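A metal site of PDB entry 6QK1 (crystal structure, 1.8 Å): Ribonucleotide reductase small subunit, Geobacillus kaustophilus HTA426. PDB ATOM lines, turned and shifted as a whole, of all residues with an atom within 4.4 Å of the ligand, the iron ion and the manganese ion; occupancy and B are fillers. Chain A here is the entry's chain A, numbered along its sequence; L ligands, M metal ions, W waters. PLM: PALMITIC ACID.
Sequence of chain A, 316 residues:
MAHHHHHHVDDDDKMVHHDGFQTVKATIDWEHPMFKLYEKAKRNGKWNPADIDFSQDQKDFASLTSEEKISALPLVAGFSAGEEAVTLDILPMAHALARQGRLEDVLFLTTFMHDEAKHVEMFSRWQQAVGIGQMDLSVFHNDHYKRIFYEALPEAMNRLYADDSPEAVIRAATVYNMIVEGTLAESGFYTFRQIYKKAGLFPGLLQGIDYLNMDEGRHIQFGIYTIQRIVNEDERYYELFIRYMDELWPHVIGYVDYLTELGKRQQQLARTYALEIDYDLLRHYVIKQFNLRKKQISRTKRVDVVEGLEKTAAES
OG1 of Thr 191 is in hydrogen-bond range of O of Ser 187 (2.8 Å).
N of Ala 185 is in hydrogen-bond range of O of Val 180 (2.8 Å).
O of Val 256 sits at hydrogen-bond distance from OG1 of Thr 260 (3.0 Å).
Leu 75 touches the ligand.
Gly 78 touches the ligand (O to C7, 3.4 Å).
CE2 of Phe 79 touches C8 of the ligand, 3.6 Å away.
Val 86 touches the ligand.
Phe 149 touches the ligand.
CG1 of Val 180 touches C2 of the ligand, 3.7 Å away.
Leu 184 touches the ligand (O to CA, 3.7 Å).
Gly 188 touches the ligand (CA to CB, 3.8 Å).
Thr 191 touches the ligand (OG1 to CD, 3.4 Å).
CE2 of Tyr 255 touches CA of the ligand, at 3.9 Å.
CG1 of Val 256 touches CE of the ligand (3.9 Å).
CD1 of Leu 282 touches CF of the ligand, at 3.8 Å.
Hydrophobic or aromatic side chains within 4 Å of the ligand: Leu 75, Phe 79, Val 86, Phe 149, Val 180, Tyr 255, Val 256 and Leu 282.
Within 4 Å of the ligand: Leu 75, Gly 78, Phe 79, Glu 83, Val 86, Glu 116, His 119, Phe 149, Val 180, Glu 181, Leu 184, Gly 188, Thr 191, Glu 216, Tyr 255, Val 256 and Leu 282.
Along chain A the residues within 4 Å of the ligand span positions 75 to 282.
The nearest printed residue that does not touch the iron ion is Phe 112 (4.3 Å).
The nearest printed residue that does not touch the manganese ion is Val 86 (4.6 Å).
An oxygen (O1) of the ligand binds the iron ion (1.8 Å).
The side-chain carboxylate (OE1) of Glu 116 binds the iron ion.
OE2 of Glu 181 binds the iron ion.
OE2 of Glu 216 binds the iron ion (2.2 Å).
The iron ion is bound by water W2, at 2.2 Å.
The iron ion is bound by a ring nitrogen (ND1) of His 219 (2.3 Å).
The manganese ion is bound by O2 of the ligand (1.7 Å), ND1 of His 119 (2.1 Å), OE2 of Glu 83 (2.1 Å), OE2 of Glu 116 (2.2 Å), water W2 (2.2 Å) and water W1 (2.4 Å).
The manganese ion has six donor atoms within binding distance.
Water W1 bridges OE1 of Glu 83 and OE1 of Glu 216.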
ATOM      1  N   LEU A  75     -16.508  -2.379 -20.010  1.00  0.00           N
ATOM      2  CA  LEU A  75     -16.969  -1.700 -18.796  1.00  0.00           C
ATOM      3  C   LEU A  75     -15.913  -0.745 -18.279  1.00  0.00           C
ATOM      4  O   LEU A  75     -16.243   0.367 -17.851  1.00  0.00           O
ATOM      5  CB  LEU A  75     -17.330  -2.749 -17.731  1.00  0.00           C
ATOM      6  CG  LEU A  75     -17.983  -2.282 -16.442  1.00  0.00           C
ATOM      7  CD1 LEU A  75     -19.284  -1.530 -16.746  1.00  0.00           C
ATOM      8  CD2 LEU A  75     -18.256  -3.487 -15.479  1.00  0.00           C
ATOM      9  N   GLY A  78     -15.944   2.311 -20.413  1.00  0.00           N
ATOM     10  CA  GLY A  78     -17.015   3.223 -20.038  1.00  0.00           C
ATOM     11  C   GLY A  78     -16.720   4.018 -18.777  1.00  0.00           C
ATOM     12  O   GLY A  78     -17.042   5.206 -18.688  1.00  0.00           O
ATOM     13  N   PHE A  79     -16.126   3.368 -17.767  1.00  0.00           N
ATOM     14  CA  PHE A  79     -15.804   4.063 -16.532  1.00  0.00           C
ATOM     15  C   PHE A  79     -14.654   5.061 -16.712  1.00  0.00           C
ATOM     16  O   PHE A  79     -14.737   6.183 -16.206  1.00  0.00           O
ATOM     17  CB  PHE A  79     -15.478   3.074 -15.424  1.00  0.00           C
ATOM     18  CG  PHE A  79     -16.655   2.776 -14.538  1.00  0.00           C
ATOM     19  CD1 PHE A  79     -17.032   3.686 -13.567  1.00  0.00           C
ATOM     20  CD2 PHE A  79     -17.397   1.616 -14.691  1.00  0.00           C
ATOM     21  CE1 PHE A  79     -18.142   3.435 -12.727  1.00  0.00           C
ATOM     22  CE2 PHE A  79     -18.475   1.351 -13.849  1.00  0.00           C
ATOM     23  CZ  PHE A  79     -18.859   2.274 -12.893  1.00  0.00           C
ATOM     24  N   GLY A  82     -15.877   8.012 -18.329  1.00  0.00           N
ATOM     25  CA  GLY A  82     -16.892   8.658 -17.526  1.00  0.00           C
ATOM     26  C   GLY A  82     -16.312   9.456 -16.391  1.00  0.00           C
ATOM     27  O   GLY A  82     -16.710  10.602 -16.150  1.00  0.00           O
ATOM     28  N   GLU A  83     -15.332   8.871 -15.665  1.00  0.00           N
ATOM     29  CA  GLU A  83     -14.663   9.564 -14.575  1.00  0.00           C
ATOM     30  C   GLU A  83     -13.924  10.790 -15.095  1.00  0.00           C
ATOM     31  O   GLU A  83     -13.873  11.832 -14.441  1.00  0.00           O
ATOM     32  CB  GLU A  83     -13.677   8.677 -13.842  1.00  0.00           C
ATOM     33  CG  GLU A  83     -14.202   7.348 -13.324  1.00  0.00           C
ATOM     34  CD  GLU A  83     -15.271   7.476 -12.256  1.00  0.00           C
ATOM     35  OE1 GLU A  83     -15.945   6.453 -11.966  1.00  0.00           O
ATOM     36  OE2 GLU A  83     -15.428   8.603 -11.726  1.00  0.00           O
ATOM     37  N   VAL A  86     -16.505  13.602 -15.956  1.00  0.00           N
ATOM     38  CA  VAL A  86     -17.105  14.303 -14.813  1.00  0.00           C
ATOM     39  C   VAL A  86     -16.047  15.118 -14.055  1.00  0.00           C
ATOM     40  O   VAL A  86     -16.358  16.187 -13.506  1.00  0.00           O
ATOM     41  CB  VAL A  86     -17.848  13.301 -13.896  1.00  0.00           C
ATOM     42  CG1 VAL A  86     -19.007  12.689 -14.617  1.00  0.00           C
ATOM     43  CG2 VAL A  86     -16.930  12.280 -13.245  1.00  0.00           C
ATOM     44  N   PHE A 112     -15.994  16.814  -3.983  1.00  0.00           N
ATOM     45  CA  PHE A 112     -16.587  16.132  -5.112  1.00  0.00           C
ATOM     46  C   PHE A 112     -15.566  16.032  -6.247  1.00  0.00           C
ATOM     47  O   PHE A 112     -15.322  14.939  -6.815  1.00  0.00           O
ATOM     48  CB  PHE A 112     -17.838  16.927  -5.527  1.00  0.00           C
ATOM     49  CG  PHE A 112     -18.759  16.276  -6.525  1.00  0.00           C
ATOM     50  CD1 PHE A 112     -20.120  16.284  -6.293  1.00  0.00           C
ATOM     51  CD2 PHE A 112     -18.331  15.809  -7.741  1.00  0.00           C
ATOM     52  CE1 PHE A 112     -21.009  15.763  -7.183  1.00  0.00           C
ATOM     53  CE2 PHE A 112     -19.214  15.282  -8.666  1.00  0.00           C
ATOM     54  CZ  PHE A 112     -20.571  15.260  -8.406  1.00  0.00           C
ATOM     55  N   GLU A 116     -13.448  12.737  -7.896  1.00  0.00           N
ATOM     56  CA  GLU A 116     -13.450  12.302  -9.291  1.00  0.00           C
ATOM     57  C   GLU A 116     -12.032  12.147  -9.810  1.00  0.00           C
ATOM     58  O   GLU A 116     -11.750  11.243 -10.595  1.00  0.00           O
ATOM     59  CB  GLU A 116     -14.245  13.274 -10.177  1.00  0.00           C
ATOM     60  CG  GLU A 116     -15.736  13.481  -9.761  1.00  0.00           C
ATOM     61  CD  GLU A 116     -16.567  12.189  -9.820  1.00  0.00           C
ATOM     62  OE1 GLU A 116     -17.774  12.272  -9.594  1.00  0.00           O
ATOM     63  OE2 GLU A 116     -16.068  11.099 -10.168  1.00  0.00           O
ATOM     64  N   HIS A 119     -10.888   8.937  -8.842  1.00  0.00           N
ATOM     65  CA  HIS A 119     -11.541   7.877  -9.613  1.00  0.00           C
ATOM     66  C   HIS A 119     -10.867   7.693 -10.979  1.00  0.00           C
ATOM     67  O   HIS A 119     -10.669   6.551 -11.442  1.00  0.00           O
ATOM     68  CB  HIS A 119     -13.005   8.155  -9.826  1.00  0.00           C
ATOM     69  CG  HIS A 119     -13.782   8.266  -8.558  1.00  0.00           C
ATOM     70  ND1 HIS A 119     -15.131   8.580  -8.517  1.00  0.00           N
ATOM     71  CD2 HIS A 119     -13.374   8.132  -7.268  1.00  0.00           C
ATOM     72  CE1 HIS A 119     -15.513   8.598  -7.241  1.00  0.00           C
ATOM     73  NE2 HIS A 119     -14.469   8.367  -6.470  1.00  0.00           N
ATOM     74  N   PHE A 149     -21.860  11.138 -22.885  1.00  0.00           N
ATOM     75  CA  PHE A 149     -20.624  11.570 -22.252  1.00  0.00           C
ATOM     76  C   PHE A 149     -19.806  12.537 -23.093  1.00  0.00           C
ATOM     77  O   PHE A 149     -19.120  13.404 -22.526  1.00  0.00           O
ATOM     78  CB  PHE A 149     -19.777  10.365 -21.902  1.00  0.00           C
ATOM     79  CG  PHE A 149     -20.283   9.605 -20.711  1.00  0.00           C
ATOM     80  CD1 PHE A 149     -19.969  10.017 -19.419  1.00  0.00           C
ATOM     81  CD2 PHE A 149     -21.103   8.497 -20.882  1.00  0.00           C
ATOM     82  CE1 PHE A 149     -20.457   9.314 -18.327  1.00  0.00           C
ATOM     83  CE2 PHE A 149     -21.570   7.799 -19.795  1.00  0.00           C
ATOM     84  CZ  PHE A 149     -21.246   8.215 -18.517  1.00  0.00           C
ATOM     85  N   VAL A 180     -25.836  10.153 -15.018  1.00  0.00           N
ATOM     86  CA  VAL A 180     -24.473   9.606 -15.136  1.00  0.00           C
ATOM     87  C   VAL A 180     -24.059   8.882 -13.846  1.00  0.00           C
ATOM     88  O   VAL A 180     -23.564   7.734 -13.883  1.00  0.00           O
ATOM     89  CB  VAL A 180     -23.495  10.733 -15.516  1.00  0.00           C
ATOM     90  CG1 VAL A 180     -22.054  10.353 -15.240  1.00  0.00           C
ATOM     91  CG2 VAL A 180     -23.732  11.121 -16.973  1.00  0.00           C
ATOM     92  N   GLU A 181     -24.232   9.533 -12.687  1.00  0.00           N
ATOM     93  CA  GLU A 181     -23.823   8.971 -11.397  1.00  0.00           C
ATOM     94  C   GLU A 181     -24.907   8.065 -10.853  1.00  0.00           C
ATOM     95  O   GLU A 181     -24.664   6.894 -10.521  1.00  0.00           O
ATOM     96  CB  GLU A 181     -23.492  10.077 -10.374  1.00  0.00           C
ATOM     97  CG  GLU A 181     -22.335  11.006 -10.780  1.00  0.00           C
ATOM     98  CD  GLU A 181     -22.036  12.068  -9.752  1.00  0.00           C
ATOM     99  OE1 GLU A 181     -22.991  12.676  -9.215  1.00  0.00           O
ATOM    100  OE2 GLU A 181     -20.850  12.262  -9.419  1.00  0.00           O
ATOM    101  N   LEU A 184     -26.125   5.320 -14.211  1.00  0.00           N
ATOM    102  CA  LEU A 184     -25.126   4.519 -14.915  1.00  0.00           C
ATOM    103  C   LEU A 184     -24.026   4.063 -13.971  1.00  0.00           C
ATOM    104  O   LEU A 184     -23.691   2.863 -13.938  1.00  0.00           O
ATOM    105  CB  LEU A 184     -24.544   5.308 -16.102  1.00  0.00           C
ATOM    106  CG  LEU A 184     -25.438   5.425 -17.311  1.00  0.00           C
ATOM    107  CD1 LEU A 184     -24.885   6.476 -18.294  1.00  0.00           C
ATOM    108  CD2 LEU A 184     -25.645   4.106 -18.044  1.00  0.00           C
ATOM    109  N   ALA A 185     -23.423   4.994 -13.216  1.00  0.00           N
ATOM    110  CA  ALA A 185     -22.340   4.609 -12.315  1.00  0.00           C
ATOM    111  C   ALA A 185     -22.789   3.538 -11.312  1.00  0.00           C
ATOM    112  O   ALA A 185     -22.098   2.525 -11.077  1.00  0.00           O
ATOM    113  CB  ALA A 185     -21.802   5.822 -11.557  1.00  0.00           C
ATOM    114  N   SER A 187     -25.139   1.398 -11.452  1.00  0.00           N
ATOM    115  CA  SER A 187     -25.366   0.126 -12.108  1.00  0.00           C
ATOM    116  C   SER A 187     -24.044  -0.521 -12.512  1.00  0.00           C
ATOM    117  O   SER A 187     -23.920  -1.740 -12.469  1.00  0.00           O
ATOM    118  CB  SER A 187     -26.269   0.279 -13.339  1.00  0.00           C
ATOM    119  OG  SER A 187     -27.525   0.846 -13.046  1.00  0.00           O
ATOM    120  N   GLY A 188     -23.041   0.275 -12.904  1.00  0.00           N
ATOM    121  CA  GLY A 188     -21.740  -0.307 -13.217  1.00  0.00           C
ATOM    122  C   GLY A 188     -21.038  -0.845 -11.996  1.00  0.00           C
ATOM    123  O   GLY A 188     -20.339  -1.863 -12.072  1.00  0.00           O
ATOM    124  N   THR A 191     -22.701  -4.121 -11.518  1.00  0.00           N
ATOM    125  CA  THR A 191     -22.258  -5.076 -12.542  1.00  0.00           C
ATOM    126  C   THR A 191     -20.866  -5.633 -12.213  1.00  0.00           C
ATOM    127  O   THR A 191     -20.634  -6.842 -12.349  1.00  0.00           O
ATOM    128  CB  THR A 191     -22.294  -4.391 -13.911  1.00  0.00           C
ATOM    129  OG1 THR A 191     -23.620  -3.967 -14.202  1.00  0.00           O
ATOM    130  CG2 THR A 191     -21.813  -5.286 -15.025  1.00  0.00           C
ATOM    131  N   GLU A 216     -19.469   8.059  -4.330  1.00  0.00           N
ATOM    132  CA  GLU A 216     -20.584   8.359  -5.219  1.00  0.00           C
ATOM    133  C   GLU A 216     -21.849   8.665  -4.437  1.00  0.00           C
ATOM    134  O   GLU A 216     -22.667   9.480  -4.863  1.00  0.00           O
ATOM    135  CB  GLU A 216     -20.849   7.173  -6.118  1.00  0.00           C
ATOM    136  CG  GLU A 216     -21.549   7.530  -7.338  1.00  0.00           C
ATOM    137  CD  GLU A 216     -20.566   8.231  -8.241  1.00  0.00           C
ATOM    138  OE1 GLU A 216     -19.648   7.545  -8.730  1.00  0.00           O
ATOM    139  OE2 GLU A 216     -20.673   9.466  -8.361  1.00  0.00           O
ATOM    140  N   HIS A 219     -21.980  12.308  -3.885  1.00  0.00           N
ATOM    141  CA  HIS A 219     -22.262  13.023  -5.133  1.00  0.00           C
ATOM    142  C   HIS A 219     -23.758  13.014  -5.461  1.00  0.00           C
ATOM    143  O   HIS A 219     -24.330  14.036  -5.825  1.00  0.00           O
ATOM    144  CB  HIS A 219     -21.451  12.399  -6.279  1.00  0.00           C
ATOM    145  CG  HIS A 219     -19.987  12.330  -6.016  1.00  0.00           C
ATOM    146  ND1 HIS A 219     -19.075  11.849  -6.937  1.00  0.00           N
ATOM    147  CD2 HIS A 219     -19.261  12.677  -4.922  1.00  0.00           C
ATOM    148  CE1 HIS A 219     -17.863  11.884  -6.405  1.00  0.00           C
ATOM    149  NE2 HIS A 219     -17.956  12.396  -5.192  1.00  0.00           N
ATOM    150  N   TYR A 255     -26.998   2.204 -24.426  1.00  0.00           N
ATOM    151  CA  TYR A 255     -25.658   1.808 -24.063  1.00  0.00           C
ATOM    152  C   TYR A 255     -25.671   0.480 -23.292  1.00  0.00           C
ATOM    153  O   TYR A 255     -24.810  -0.388 -23.508  1.00  0.00           O
ATOM    154  CB  TYR A 255     -24.999   2.914 -23.256  1.00  0.00           C
ATOM    155  CG  TYR A 255     -23.627   2.567 -22.730  1.00  0.00           C
ATOM    156  CD1 TYR A 255     -22.589   2.180 -23.587  1.00  0.00           C
ATOM    157  CD2 TYR A 255     -23.348   2.622 -21.362  1.00  0.00           C
ATOM    158  CE1 TYR A 255     -21.319   1.870 -23.080  1.00  0.00           C
ATOM    159  CE2 TYR A 255     -22.078   2.311 -20.855  1.00  0.00           C
ATOM    160  CZ  TYR A 255     -21.066   1.950 -21.721  1.00  0.00           C
ATOM    161  OH  TYR A 255     -19.821   1.635 -21.152  1.00  0.00           O
ATOM    162  N   VAL A 256     -26.626   0.316 -22.380  1.00  0.00           N
ATOM    163  CA  VAL A 256     -26.766  -0.932 -21.651  1.00  0.00           C
ATOM    164  C   VAL A 256     -26.964  -2.089 -22.624  1.00  0.00           C
ATOM    165  O   VAL A 256     -26.333  -3.150 -22.484  1.00  0.00           O
ATOM    166  CB  VAL A 256     -27.925  -0.844 -20.629  1.00  0.00           C
ATOM    167  CG1 VAL A 256     -28.187  -2.211 -20.013  1.00  0.00           C
ATOM    168  CG2 VAL A 256     -27.600   0.170 -19.543  1.00  0.00           C
ATOM    169  N   LEU A 259     -23.625  -2.956 -24.392  1.00  0.00           N
ATOM    170  CA  LEU A 259     -22.739  -3.732 -23.509  1.00  0.00           C
ATOM    171  C   LEU A 259     -23.254  -5.147 -23.288  1.00  0.00           C
ATOM    172  O   LEU A 259     -22.461  -6.087 -23.175  1.00  0.00           O
ATOM    173  CB  LEU A 259     -22.592  -3.047 -22.163  1.00  0.00           C
ATOM    174  CG  LEU A 259     -21.806  -1.757 -22.100  1.00  0.00           C
ATOM    175  CD1 LEU A 259     -21.955  -1.288 -20.649  1.00  0.00           C
ATOM    176  CD2 LEU A 259     -20.343  -1.957 -22.510  1.00  0.00           C
ATOM    177  N   THR A 260     -24.571  -5.299 -23.168  1.00  0.00           N
ATOM    178  CA  THR A 260     -25.181  -6.626 -23.037  1.00  0.00           C
ATOM    179  C   THR A 260     -24.885  -7.495 -24.253  1.00  0.00           C
ATOM    180  O   THR A 260     -24.466  -8.649 -24.124  1.00  0.00           O
ATOM    181  CB  THR A 260     -26.677  -6.469 -22.827  1.00  0.00           C
ATOM    182  OG1 THR A 260     -26.911  -5.965 -21.502  1.00  0.00           O
ATOM    183  CG2 THR A 260     -27.414  -7.792 -23.008  1.00  0.00           C
ATOM    184  N   LEU A 282     -29.148  -7.532 -14.696  1.00  0.00           N
ATOM    185  CA  LEU A 282     -28.408  -6.284 -14.826  1.00  0.00           C
ATOM    186  C   LEU A 282     -29.266  -5.210 -15.460  1.00  0.00           C
ATOM    187  O   LEU A 282     -29.343  -4.077 -14.962  1.00  0.00           O
ATOM    188  CB  LEU A 282     -27.139  -6.514 -15.643  1.00  0.00           C
ATOM    189  CG  LEU A 282     -26.035  -7.409 -15.081  1.00  0.00           C
ATOM    190  CD1 LEU A 282     -24.805  -7.410 -16.007  1.00  0.00           C
ATOM    191  CD2 LEU A 282     -25.650  -7.032 -13.644  1.00  0.00           C
ATOM    192  N   VAL A 286     -30.693  -1.515 -13.760  1.00  0.00           N
ATOM    193  CA  VAL A 286     -30.593  -0.189 -14.392  1.00  0.00           C
ATOM    194  C   VAL A 286     -31.945   0.485 -14.380  1.00  0.00           C
ATOM    195  O   VAL A 286     -32.072   1.651 -13.984  1.00  0.00           O
ATOM    196  CB  VAL A 286     -30.066  -0.315 -15.837  1.00  0.00           C
ATOM    197  CG1 VAL A 286     -30.161   1.055 -16.579  1.00  0.00           C
ATOM    198  CG2 VAL A 286     -28.669  -0.790 -15.854  1.00  0.00           C
HETATM  199  C1  PLM L   1     -18.804   9.536 -11.539  1.00  0.00           C
HETATM  200  O1  PLM L   1     -19.425  10.442 -10.780  1.00  0.00           O
HETATM  201  O2  PLM L   1     -17.723   8.939 -11.269  1.00  0.00           O
HETATM  202  C2  PLM L   1     -19.487   9.106 -12.928  1.00  0.00           C
HETATM  203  C3  PLM L   1     -18.913   7.867 -13.669  1.00  0.00           C
HETATM  204  C4  PLM L   1     -19.730   7.348 -14.824  1.00  0.00           C
HETATM  205  C5  PLM L   1     -19.437   5.869 -15.240  1.00  0.00           C
HETATM  206  C6  PLM L   1     -19.936   5.517 -16.577  1.00  0.00           C
HETATM  207  C7  PLM L   1     -19.725   4.021 -17.012  1.00  0.00           C
HETATM  208  C8  PLM L   1     -20.564   3.073 -16.228  1.00  0.00           C
HETATM  209  C9  PLM L   1     -20.852   1.731 -16.930  1.00  0.00           C
HETATM  210  CA  PLM L   1     -22.363   1.462 -17.096  1.00  0.00           C
HETATM  211  CB  PLM L   1     -22.723   0.023 -16.895  1.00  0.00           C
HETATM  212  CC  PLM L   1     -24.239  -0.241 -16.821  1.00  0.00           C
HETATM  213  CD  PLM L   1     -24.513  -1.744 -16.630  1.00  0.00           C
HETATM  214  CE  PLM L   1     -24.854  -2.519 -17.922  1.00  0.00           C
HETATM  215  CF  PLM L   1     -24.857  -4.059 -17.788  1.00  0.00           C
HETATM  216  CG  PLM L   1     -23.987  -4.791 -18.831  1.00  0.00           C
HETATM  217 FE    FE M   1     -19.266  10.980  -9.093  1.00  0.00          FE
HETATM  218 MN    MN M   2     -16.585   9.012  -9.997  1.00  0.00          MN
HETATM  219  O   HOH W   1     -17.374   6.784  -9.932  1.00  0.00           O
HETATM  220  O   HOH W   2     -18.004   9.337  -8.317  1.00  0.00           O
